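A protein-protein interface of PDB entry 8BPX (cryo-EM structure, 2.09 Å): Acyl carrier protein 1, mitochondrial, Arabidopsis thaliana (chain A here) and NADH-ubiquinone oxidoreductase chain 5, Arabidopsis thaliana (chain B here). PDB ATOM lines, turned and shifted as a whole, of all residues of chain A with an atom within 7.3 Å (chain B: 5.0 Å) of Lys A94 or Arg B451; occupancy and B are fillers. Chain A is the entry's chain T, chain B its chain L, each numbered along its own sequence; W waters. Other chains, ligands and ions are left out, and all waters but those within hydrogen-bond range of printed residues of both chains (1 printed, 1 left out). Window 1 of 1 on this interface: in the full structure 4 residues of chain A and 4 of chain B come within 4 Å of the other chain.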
ATOM      1  N   ARG A  49     -36.508 -18.861 -31.757  1.00  0.00           N
ATOM      2  CA  ARG A  49     -36.701 -17.963 -30.605  1.00  0.00           C
ATOM      3  C   ARG A  49     -36.999 -16.501 -31.041  1.00  0.00           C
ATOM      4  O   ARG A  49     -37.686 -15.824 -30.305  1.00  0.00           O
ATOM      5  CB  ARG A  49     -35.510 -18.081 -29.640  1.00  0.00           C
ATOM      6  CG  ARG A  49     -35.155 -19.445 -29.093  1.00  0.00           C
ATOM      7  CD  ARG A  49     -34.274 -19.005 -27.951  1.00  0.00           C
ATOM      8  NE  ARG A  49     -32.863 -19.333 -27.994  1.00  0.00           N
ATOM      9  CZ  ARG A  49     -31.937 -18.706 -27.291  1.00  0.00           C
ATOM     10  NH1 ARG A  49     -32.255 -17.671 -26.534  1.00  0.00           N
ATOM     11  NH2 ARG A  49     -30.678 -19.082 -27.386  1.00  0.00           N
ATOM     12  N   ALA A  88     -37.251  -6.610 -26.729  1.00  0.00           N
ATOM     13  CA  ALA A  88     -37.596  -7.958 -26.286  1.00  0.00           C
ATOM     14  C   ALA A  88     -36.600  -8.990 -26.808  1.00  0.00           C
ATOM     15  O   ALA A  88     -36.235  -9.924 -26.089  1.00  0.00           O
ATOM     16  CB  ALA A  88     -39.014  -8.310 -26.724  1.00  0.00           C
ATOM     17  N   ILE A  89     -36.153  -8.837 -28.056  1.00  0.00           N
ATOM     18  CA  ILE A  89     -35.116  -9.718 -28.599  1.00  0.00           C
ATOM     19  C   ILE A  89     -33.818  -9.554 -27.813  1.00  0.00           C
ATOM     20  O   ILE A  89     -33.122 -10.534 -27.501  1.00  0.00           O
ATOM     21  CB  ILE A  89     -34.917  -9.436 -30.100  1.00  0.00           C
ATOM     22  CG1 ILE A  89     -36.096  -9.978 -30.908  1.00  0.00           C
ATOM     23  CG2 ILE A  89     -33.610 -10.031 -30.604  1.00  0.00           C
ATOM     24  CD1 ILE A  89     -36.292  -9.290 -32.246  1.00  0.00           C
ATOM     25  N   GLU A  90     -33.475  -8.303 -27.489  1.00  0.00           N
ATOM     26  CA  GLU A  90     -32.317  -8.003 -26.655  1.00  0.00           C
ATOM     27  C   GLU A  90     -32.370  -8.776 -25.345  1.00  0.00           C
ATOM     28  O   GLU A  90     -31.394  -9.419 -24.947  1.00  0.00           O
ATOM     29  CB  GLU A  90     -32.269  -6.500 -26.368  1.00  0.00           C
ATOM     30  CG  GLU A  90     -31.686  -5.632 -27.461  1.00  0.00           C
ATOM     31  CD  GLU A  90     -30.182  -5.585 -27.403  1.00  0.00           C
ATOM     32  OE1 GLU A  90     -29.556  -6.628 -27.662  1.00  0.00           O
ATOM     33  OE2 GLU A  90     -29.622  -4.510 -27.102  1.00  0.00           O
ATOM     34  N   GLU A  91     -33.530  -8.875 -24.672  1.00  0.00           N
ATOM     35  CA  GLU A  91     -33.642  -9.528 -23.356  1.00  0.00           C
ATOM     36  C   GLU A  91     -33.619 -11.018 -23.620  1.00  0.00           C
ATOM     37  O   GLU A  91     -33.046 -11.749 -22.847  1.00  0.00           O
ATOM     38  CB  GLU A  91     -34.918  -9.144 -22.585  1.00  0.00           C
ATOM     39  CG  GLU A  91     -34.896  -7.776 -21.945  1.00  0.00           C
ATOM     40  CD  GLU A  91     -35.921  -7.623 -20.831  1.00  0.00           C
ATOM     41  OE1 GLU A  91     -36.109  -6.497 -20.341  1.00  0.00           O
ATOM     42  OE2 GLU A  91     -36.520  -8.645 -20.445  1.00  0.00           O
ATOM     43  N   GLU A  92     -34.186 -11.394 -24.731  1.00  0.00           N
ATOM     44  CA  GLU A  92     -34.297 -12.827 -24.957  1.00  0.00           C
ATOM     45  C   GLU A  92     -32.929 -13.467 -25.162  1.00  0.00           C
ATOM     46  O   GLU A  92     -32.699 -14.597 -24.719  1.00  0.00           O
ATOM     47  CB  GLU A  92     -35.212 -13.094 -26.153  1.00  0.00           C
ATOM     48  CG  GLU A  92     -35.042 -14.465 -26.755  1.00  0.00           C
ATOM     49  CD  GLU A  92     -35.648 -15.530 -25.874  1.00  0.00           C
ATOM     50  OE1 GLU A  92     -36.366 -15.179 -24.915  1.00  0.00           O
ATOM     51  OE2 GLU A  92     -35.398 -16.721 -26.118  1.00  0.00           O
ATOM     52  N   PHE A  93     -31.951 -12.781 -25.786  1.00  0.00           N
ATOM     53  CA  PHE A  93     -30.622 -13.394 -26.036  1.00  0.00           C
ATOM     54  C   PHE A  93     -29.564 -12.776 -25.102  1.00  0.00           C
ATOM     55  O   PHE A  93     -28.422 -13.185 -25.253  1.00  0.00           O
ATOM     56  CB  PHE A  93     -30.238 -13.327 -27.538  1.00  0.00           C
ATOM     57  CG  PHE A  93     -31.056 -14.200 -28.453  1.00  0.00           C
ATOM     58  CD1 PHE A  93     -30.723 -15.528 -28.652  1.00  0.00           C
ATOM     59  CD2 PHE A  93     -32.160 -13.694 -29.117  1.00  0.00           C
ATOM     60  CE1 PHE A  93     -31.469 -16.327 -29.500  1.00  0.00           C
ATOM     61  CE2 PHE A  93     -32.913 -14.496 -29.957  1.00  0.00           C
ATOM     62  CZ  PHE A  93     -32.563 -15.810 -30.148  1.00  0.00           C
ATOM     63  N   LYS A  94     -29.929 -11.845 -24.183  1.00  0.00           N
ATOM     64  CA  LYS A  94     -28.934 -11.126 -23.320  1.00  0.00           C
ATOM     65  C   LYS A  94     -27.897 -10.395 -24.196  1.00  0.00           C
ATOM     66  O   LYS A  94     -26.726 -10.572 -23.986  1.00  0.00           O
ATOM     67  CB  LYS A  94     -28.347 -11.933 -22.144  1.00  0.00           C
ATOM     68  CG  LYS A  94     -27.868 -11.071 -20.991  1.00  0.00           C
ATOM     69  CD  LYS A  94     -27.035 -11.741 -19.926  1.00  0.00           C
ATOM     70  CE  LYS A  94     -26.637 -10.743 -18.852  1.00  0.00           C
ATOM     71  NZ  LYS A  94     -25.854 -11.339 -17.746  1.00  0.00           N
ATOM     72  N   LEU A  95     -28.349  -9.463 -25.014  1.00  0.00           N
ATOM     73  CA  LEU A  95     -27.409  -8.678 -25.797  1.00  0.00           C
ATOM     74  C   LEU A  95     -27.616  -7.201 -25.503  1.00  0.00           C
ATOM     75  O   LEU A  95     -28.663  -6.783 -25.003  1.00  0.00           O
ATOM     76  CB  LEU A  95     -27.552  -8.937 -27.301  1.00  0.00           C
ATOM     77  CG  LEU A  95     -27.687 -10.387 -27.758  1.00  0.00           C
ATOM     78  CD1 LEU A  95     -28.263 -10.459 -29.166  1.00  0.00           C
ATOM     79  CD2 LEU A  95     -26.367 -11.121 -27.656  1.00  0.00           C
ATOM     80  N   GLU A  96     -26.594  -6.410 -25.803  1.00  0.00           N
ATOM     81  CA  GLU A  96     -26.666  -4.955 -25.700  1.00  0.00           C
ATOM     82  C   GLU A  96     -26.331  -4.396 -27.079  1.00  0.00           C
ATOM     83  O   GLU A  96     -25.163  -4.153 -27.390  1.00  0.00           O
ATOM     84  CB  GLU A  96     -25.725  -4.419 -24.625  1.00  0.00           C
ATOM     85  CG  GLU A  96     -25.970  -2.963 -24.265  1.00  0.00           C
ATOM     86  CD  GLU A  96     -25.723  -2.663 -22.792  1.00  0.00           C
ATOM     87  OE1 GLU A  96     -26.165  -3.455 -21.940  1.00  0.00           O
ATOM     88  OE2 GLU A  96     -25.099  -1.629 -22.485  1.00  0.00           O
ATOM     89  N   ILE A  97     -27.352  -4.215 -27.902  1.00  0.00           N
ATOM     90  CA  ILE A  97     -27.157  -3.679 -29.250  1.00  0.00           C
ATOM     91  C   ILE A  97     -26.938  -2.172 -29.155  1.00  0.00           C
ATOM     92  O   ILE A  97     -27.677  -1.491 -28.430  1.00  0.00           O
ATOM     93  CB  ILE A  97     -28.354  -4.006 -30.135  1.00  0.00           C
ATOM     94  CG1 ILE A  97     -28.480  -5.516 -30.304  1.00  0.00           C
ATOM     95  CG2 ILE A  97     -28.204  -3.348 -31.499  1.00  0.00           C
ATOM     96  CD1 ILE A  97     -29.815  -5.972 -30.826  1.00  0.00           C
ATOM     97  N   HIS A 118     -23.917 -12.439 -33.980  1.00  0.00           N
ATOM     98  CA  HIS A 118     -23.299 -11.965 -32.752  1.00  0.00           C
ATOM     99  C   HIS A 118     -22.642 -13.138 -32.034  1.00  0.00           C
ATOM    100  O   HIS A 118     -23.304 -14.144 -31.764  1.00  0.00           O
ATOM    101  CB  HIS A 118     -24.309 -11.286 -31.833  1.00  0.00           C
ATOM    102  CG  HIS A 118     -23.683 -10.311 -30.889  1.00  0.00           C
ATOM    103  ND1 HIS A 118     -22.476  -9.706 -31.148  1.00  0.00           N
ATOM    104  CD2 HIS A 118     -24.066  -9.874 -29.668  1.00  0.00           C
ATOM    105  CE1 HIS A 118     -22.153  -8.916 -30.140  1.00  0.00           C
ATOM    106  NE2 HIS A 118     -23.100  -9.004 -29.227  1.00  0.00           N
ATOM    107  N   MET A 120     -21.681 -13.415 -28.963  1.00  0.00           N
ATOM    108  CA  MET A 120     -22.049 -13.565 -27.565  1.00  0.00           C
ATOM    109  C   MET A 120     -23.513 -13.933 -27.375  1.00  0.00           C
ATOM    110  O   MET A 120     -23.984 -13.968 -26.235  1.00  0.00           O
ATOM    111  CB  MET A 120     -21.729 -12.289 -26.789  1.00  0.00           C
ATOM    112  CG  MET A 120     -20.252 -12.114 -26.502  1.00  0.00           C
ATOM    113  SD  MET A 120     -19.650 -13.141 -25.154  1.00  0.00           S
ATOM    114  CE  MET A 120     -21.071 -13.215 -24.075  1.00  0.00           C
ATOM    115  N   SER A 121     -24.259 -14.245 -28.429  1.00  0.00           N
ATOM    116  CA  SER A 121     -25.683 -14.663 -28.268  1.00  0.00           C
ATOM    117  C   SER A 121     -25.814 -16.056 -27.636  1.00  0.00           C
ATOM    118  O   SER A 121     -26.794 -16.285 -26.913  1.00  0.00           O
ATOM    119  CB  SER A 121     -26.405 -14.589 -29.579  1.00  0.00           C
ATOM    120  OG  SER A 121     -26.248 -13.315 -30.180  1.00  0.00           O
ATOM    121  N   MET B 359     -23.780 -17.019 -12.040  1.00  0.00           N
ATOM    122  CA  MET B 359     -24.646 -16.205 -12.880  1.00  0.00           C
ATOM    123  C   MET B 359     -23.914 -15.640 -14.093  1.00  0.00           C
ATOM    124  O   MET B 359     -24.293 -14.584 -14.607  1.00  0.00           O
ATOM    125  CB  MET B 359     -25.257 -15.077 -12.053  1.00  0.00           C
ATOM    126  CG  MET B 359     -26.329 -15.522 -11.078  1.00  0.00           C
ATOM    127  SD  MET B 359     -27.450 -16.741 -11.771  1.00  0.00           S
ATOM    128  CE  MET B 359     -28.700 -15.655 -12.450  1.00  0.00           C
ATOM    129  N   GLU B 362     -22.637 -12.008 -13.863  1.00  0.00           N
ATOM    130  CA  GLU B 362     -23.564 -10.920 -13.588  1.00  0.00           C
ATOM    131  C   GLU B 362     -23.356 -10.450 -12.155  1.00  0.00           C
ATOM    132  O   GLU B 362     -23.324 -11.260 -11.224  1.00  0.00           O
ATOM    133  CB  GLU B 362     -25.010 -11.367 -13.809  1.00  0.00           C
ATOM    134  CG  GLU B 362     -26.042 -10.288 -13.534  1.00  0.00           C
ATOM    135  CD  GLU B 362     -25.897  -9.092 -14.461  1.00  0.00           C
ATOM    136  OE1 GLU B 362     -26.093  -9.252 -15.684  1.00  0.00           O
ATOM    137  OE2 GLU B 362     -25.586  -7.991 -13.968  1.00  0.00           O
ATOM    138  N   PHE B 449     -31.957 -12.907 -16.537  1.00  0.00           N
ATOM    139  CA  PHE B 449     -32.066 -13.304 -17.945  1.00  0.00           C
ATOM    140  C   PHE B 449     -32.217 -14.830 -17.953  1.00  0.00           C
ATOM    141  O   PHE B 449     -31.574 -15.476 -17.140  1.00  0.00           O
ATOM    142  CB  PHE B 449     -30.795 -12.781 -18.640  1.00  0.00           C
ATOM    143  CG  PHE B 449     -30.700 -11.291 -18.844  1.00  0.00           C
ATOM    144  CD1 PHE B 449     -30.003 -10.491 -17.956  1.00  0.00           C
ATOM    145  CD2 PHE B 449     -31.255 -10.686 -19.960  1.00  0.00           C
ATOM    146  CE1 PHE B 449     -29.886  -9.125 -18.155  1.00  0.00           C
ATOM    147  CE2 PHE B 449     -31.142  -9.319 -20.160  1.00  0.00           C
ATOM    148  CZ  PHE B 449     -30.456  -8.539 -19.259  1.00  0.00           C
ATOM    149  N   GLY B 450     -33.075 -15.382 -18.788  1.00  0.00           N
ATOM    150  CA  GLY B 450     -33.186 -16.831 -18.917  1.00  0.00           C
ATOM    151  C   GLY B 450     -31.884 -17.511 -19.228  1.00  0.00           C
ATOM    152  O   GLY B 450     -31.636 -18.563 -18.626  1.00  0.00           O
ATOM    153  N   ARG B 451     -31.039 -16.909 -20.068  1.00  0.00           N
ATOM    154  CA  ARG B 451     -29.772 -17.586 -20.457  1.00  0.00           C
ATOM    155  C   ARG B 451     -28.883 -17.744 -19.213  1.00  0.00           C
ATOM    156  O   ARG B 451     -28.081 -18.694 -19.189  1.00  0.00           O
ATOM    157  CB  ARG B 451     -29.065 -16.847 -21.601  1.00  0.00           C
ATOM    158  CG  ARG B 451     -27.768 -17.479 -22.085  1.00  0.00           C
ATOM    159  CD  ARG B 451     -27.106 -16.788 -23.262  1.00  0.00           C
ATOM    160  NE  ARG B 451     -26.635 -15.440 -22.980  1.00  0.00           N
ATOM    161  CZ  ARG B 451     -25.473 -15.154 -22.403  1.00  0.00           C
ATOM    162  NH1 ARG B 451     -24.660 -16.127 -22.030  1.00  0.00           N
ATOM    163  NH2 ARG B 451     -25.134 -13.895 -22.188  1.00  0.00           N
ATOM    164  N   ASP B 452     -29.030 -16.860 -18.216  1.00  0.00           N
ATOM    165  CA  ASP B 452     -28.226 -16.984 -16.976  1.00  0.00           C
ATOM    166  C   ASP B 452     -28.751 -18.145 -16.102  1.00  0.00           C
ATOM    167  O   ASP B 452     -27.956 -18.940 -15.727  1.00  0.00           O
ATOM    168  CB  ASP B 452     -28.084 -15.624 -16.262  1.00  0.00           C
ATOM    169  CG  ASP B 452     -27.254 -14.594 -16.995  1.00  0.00           C
ATOM    170  OD1 ASP B 452     -26.215 -14.961 -17.561  1.00  0.00           O
ATOM    171  OD2 ASP B 452     -27.651 -13.438 -16.980  1.00  0.00           O
ATOM    172  N   ILE B 453     -30.058 -18.281 -15.956  1.00  0.00           N
ATOM    173  CA  ILE B 453     -30.720 -19.305 -15.082  1.00  0.00           C
ATOM    174  C   ILE B 453     -30.432 -20.696 -15.605  1.00  0.00           C
ATOM    175  O   ILE B 453     -30.059 -21.535 -14.831  1.00  0.00           O
ATOM    176  CB  ILE B 453     -32.224 -18.936 -15.099  1.00  0.00           C
ATOM    177  CG1 ILE B 453     -32.535 -17.794 -14.134  1.00  0.00           C
ATOM    178  CG2 ILE B 453     -33.101 -20.147 -14.833  1.00  0.00           C
ATOM    179  CD1 ILE B 453     -31.909 -17.976 -12.779  1.00  0.00           C
ATOM    180  N   SER B 454     -30.367 -20.833 -16.910  1.00  0.00           N
ATOM    181  CA  SER B 454     -30.242 -22.102 -17.624  1.00  0.00           C
ATOM    182  C   SER B 454     -28.794 -22.587 -17.713  1.00  0.00           C
ATOM    183  O   SER B 454     -28.608 -23.674 -18.104  1.00  0.00           O
ATOM    184  CB  SER B 454     -30.916 -21.838 -18.948  1.00  0.00           C
ATOM    185  OG  SER B 454     -32.299 -22.071 -18.846  1.00  0.00           O
ATOM    186  N   ARG B 455     -27.868 -21.843 -17.154  1.00  0.00           N
ATOM    187  CA  ARG B 455     -26.439 -22.183 -17.153  1.00  0.00           C
ATOM    188  C   ARG B 455     -25.892 -22.119 -15.704  1.00  0.00           C
ATOM    189  O   ARG B 455     -24.682 -22.148 -15.589  1.00  0.00           O
ATOM    190  CB  ARG B 455     -25.739 -21.213 -18.091  1.00  0.00           C
ATOM    191  CG  ARG B 455     -26.105 -21.316 -19.560  1.00  0.00           C
ATOM    192  CD  ARG B 455     -25.282 -20.306 -20.329  1.00  0.00           C
ATOM    193  NE  ARG B 455     -24.173 -20.915 -21.038  1.00  0.00           N
ATOM    194  CZ  ARG B 455     -24.099 -21.037 -22.361  1.00  0.00           C
ATOM    195  NH1 ARG B 455     -25.066 -20.565 -23.129  1.00  0.00           N
ATOM    196  NH2 ARG B 455     -23.048 -21.619 -22.910  1.00  0.00           N
HETATM  197  O   HOH W   1     -31.809 -14.537 -21.581  1.00  0.00           O
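Among the printed residues, pairs that only touch across the chains: Glu A91 with Phe B449, Phe A93 with Arg B451, Lys A94 with Phe B449, Lys A94 with Arg B451 and Ser A121 with Arg B451.
The backbone carbonyl oxygen (O) of His A118 lies close to the side-chain hydroxyl (OG) of Ser A121 (3.4 Å).
Printed residues of chain B within 4 Å of Phe A93: Arg B451. Of the printed residues of chain B, Lys A94 touches Glu B362, Phe B449, Arg B451 and Asp B452. His A118 touches none of the printed residues of chain B. Met A120 touches none of the printed residues of chain B. Of the printed residues of chain B, Ser A121 touches Arg B451. Printed residues of chain A within 4 Å of Glu B362: Lys A94 (2.9 Å). Printed residues of chain A within 4 Å of Phe B449: Glu A91 and Lys A94. Arg B451 touches just these residues of chain A: Phe A93, Lys A94 and Ser A121. Of the printed residues of chain A, Asp B452 touches Lys A94 (2.9 Å). The nearest residue of chain B that does not touch Lys A94 is Met B359 (4.8 Å).
OE1 of Glu B362 is in salt-bridge range of NZ of Lys A94. OD2 of Asp B452 is in salt-bridge range of NZ of Lys A94 (2.9 Å).
Printed residues of chain A that touch a printed residue of chain B: Glu A91, Phe A93, Lys A94 and Ser A121. Hydrophobic or aromatic side chains of chain B that line the printed part of chain A: Phe B449. Among the printed residues, 7 pairs touch across the chains. Among the printed residues, Asp or Glu carboxylates within 4 Å of a Lys or Arg side-chain nitrogen of the other chain: Lys A94 with Glu B362 (2.9 Å) and Lys A94 with Asp B452 (2.9 Å).
Water W1 lies within hydrogen-bond range of the backbone NH (N) of Arg B451 (2.9 Å), the backbone NH (N) of Gly B450 (3.2 Å), the backbone carbonyl oxygen (O) of Glu A92 (3.3 Å) and the backbone carbonyl oxygen (O) of Glu A91 (3.3 Å).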
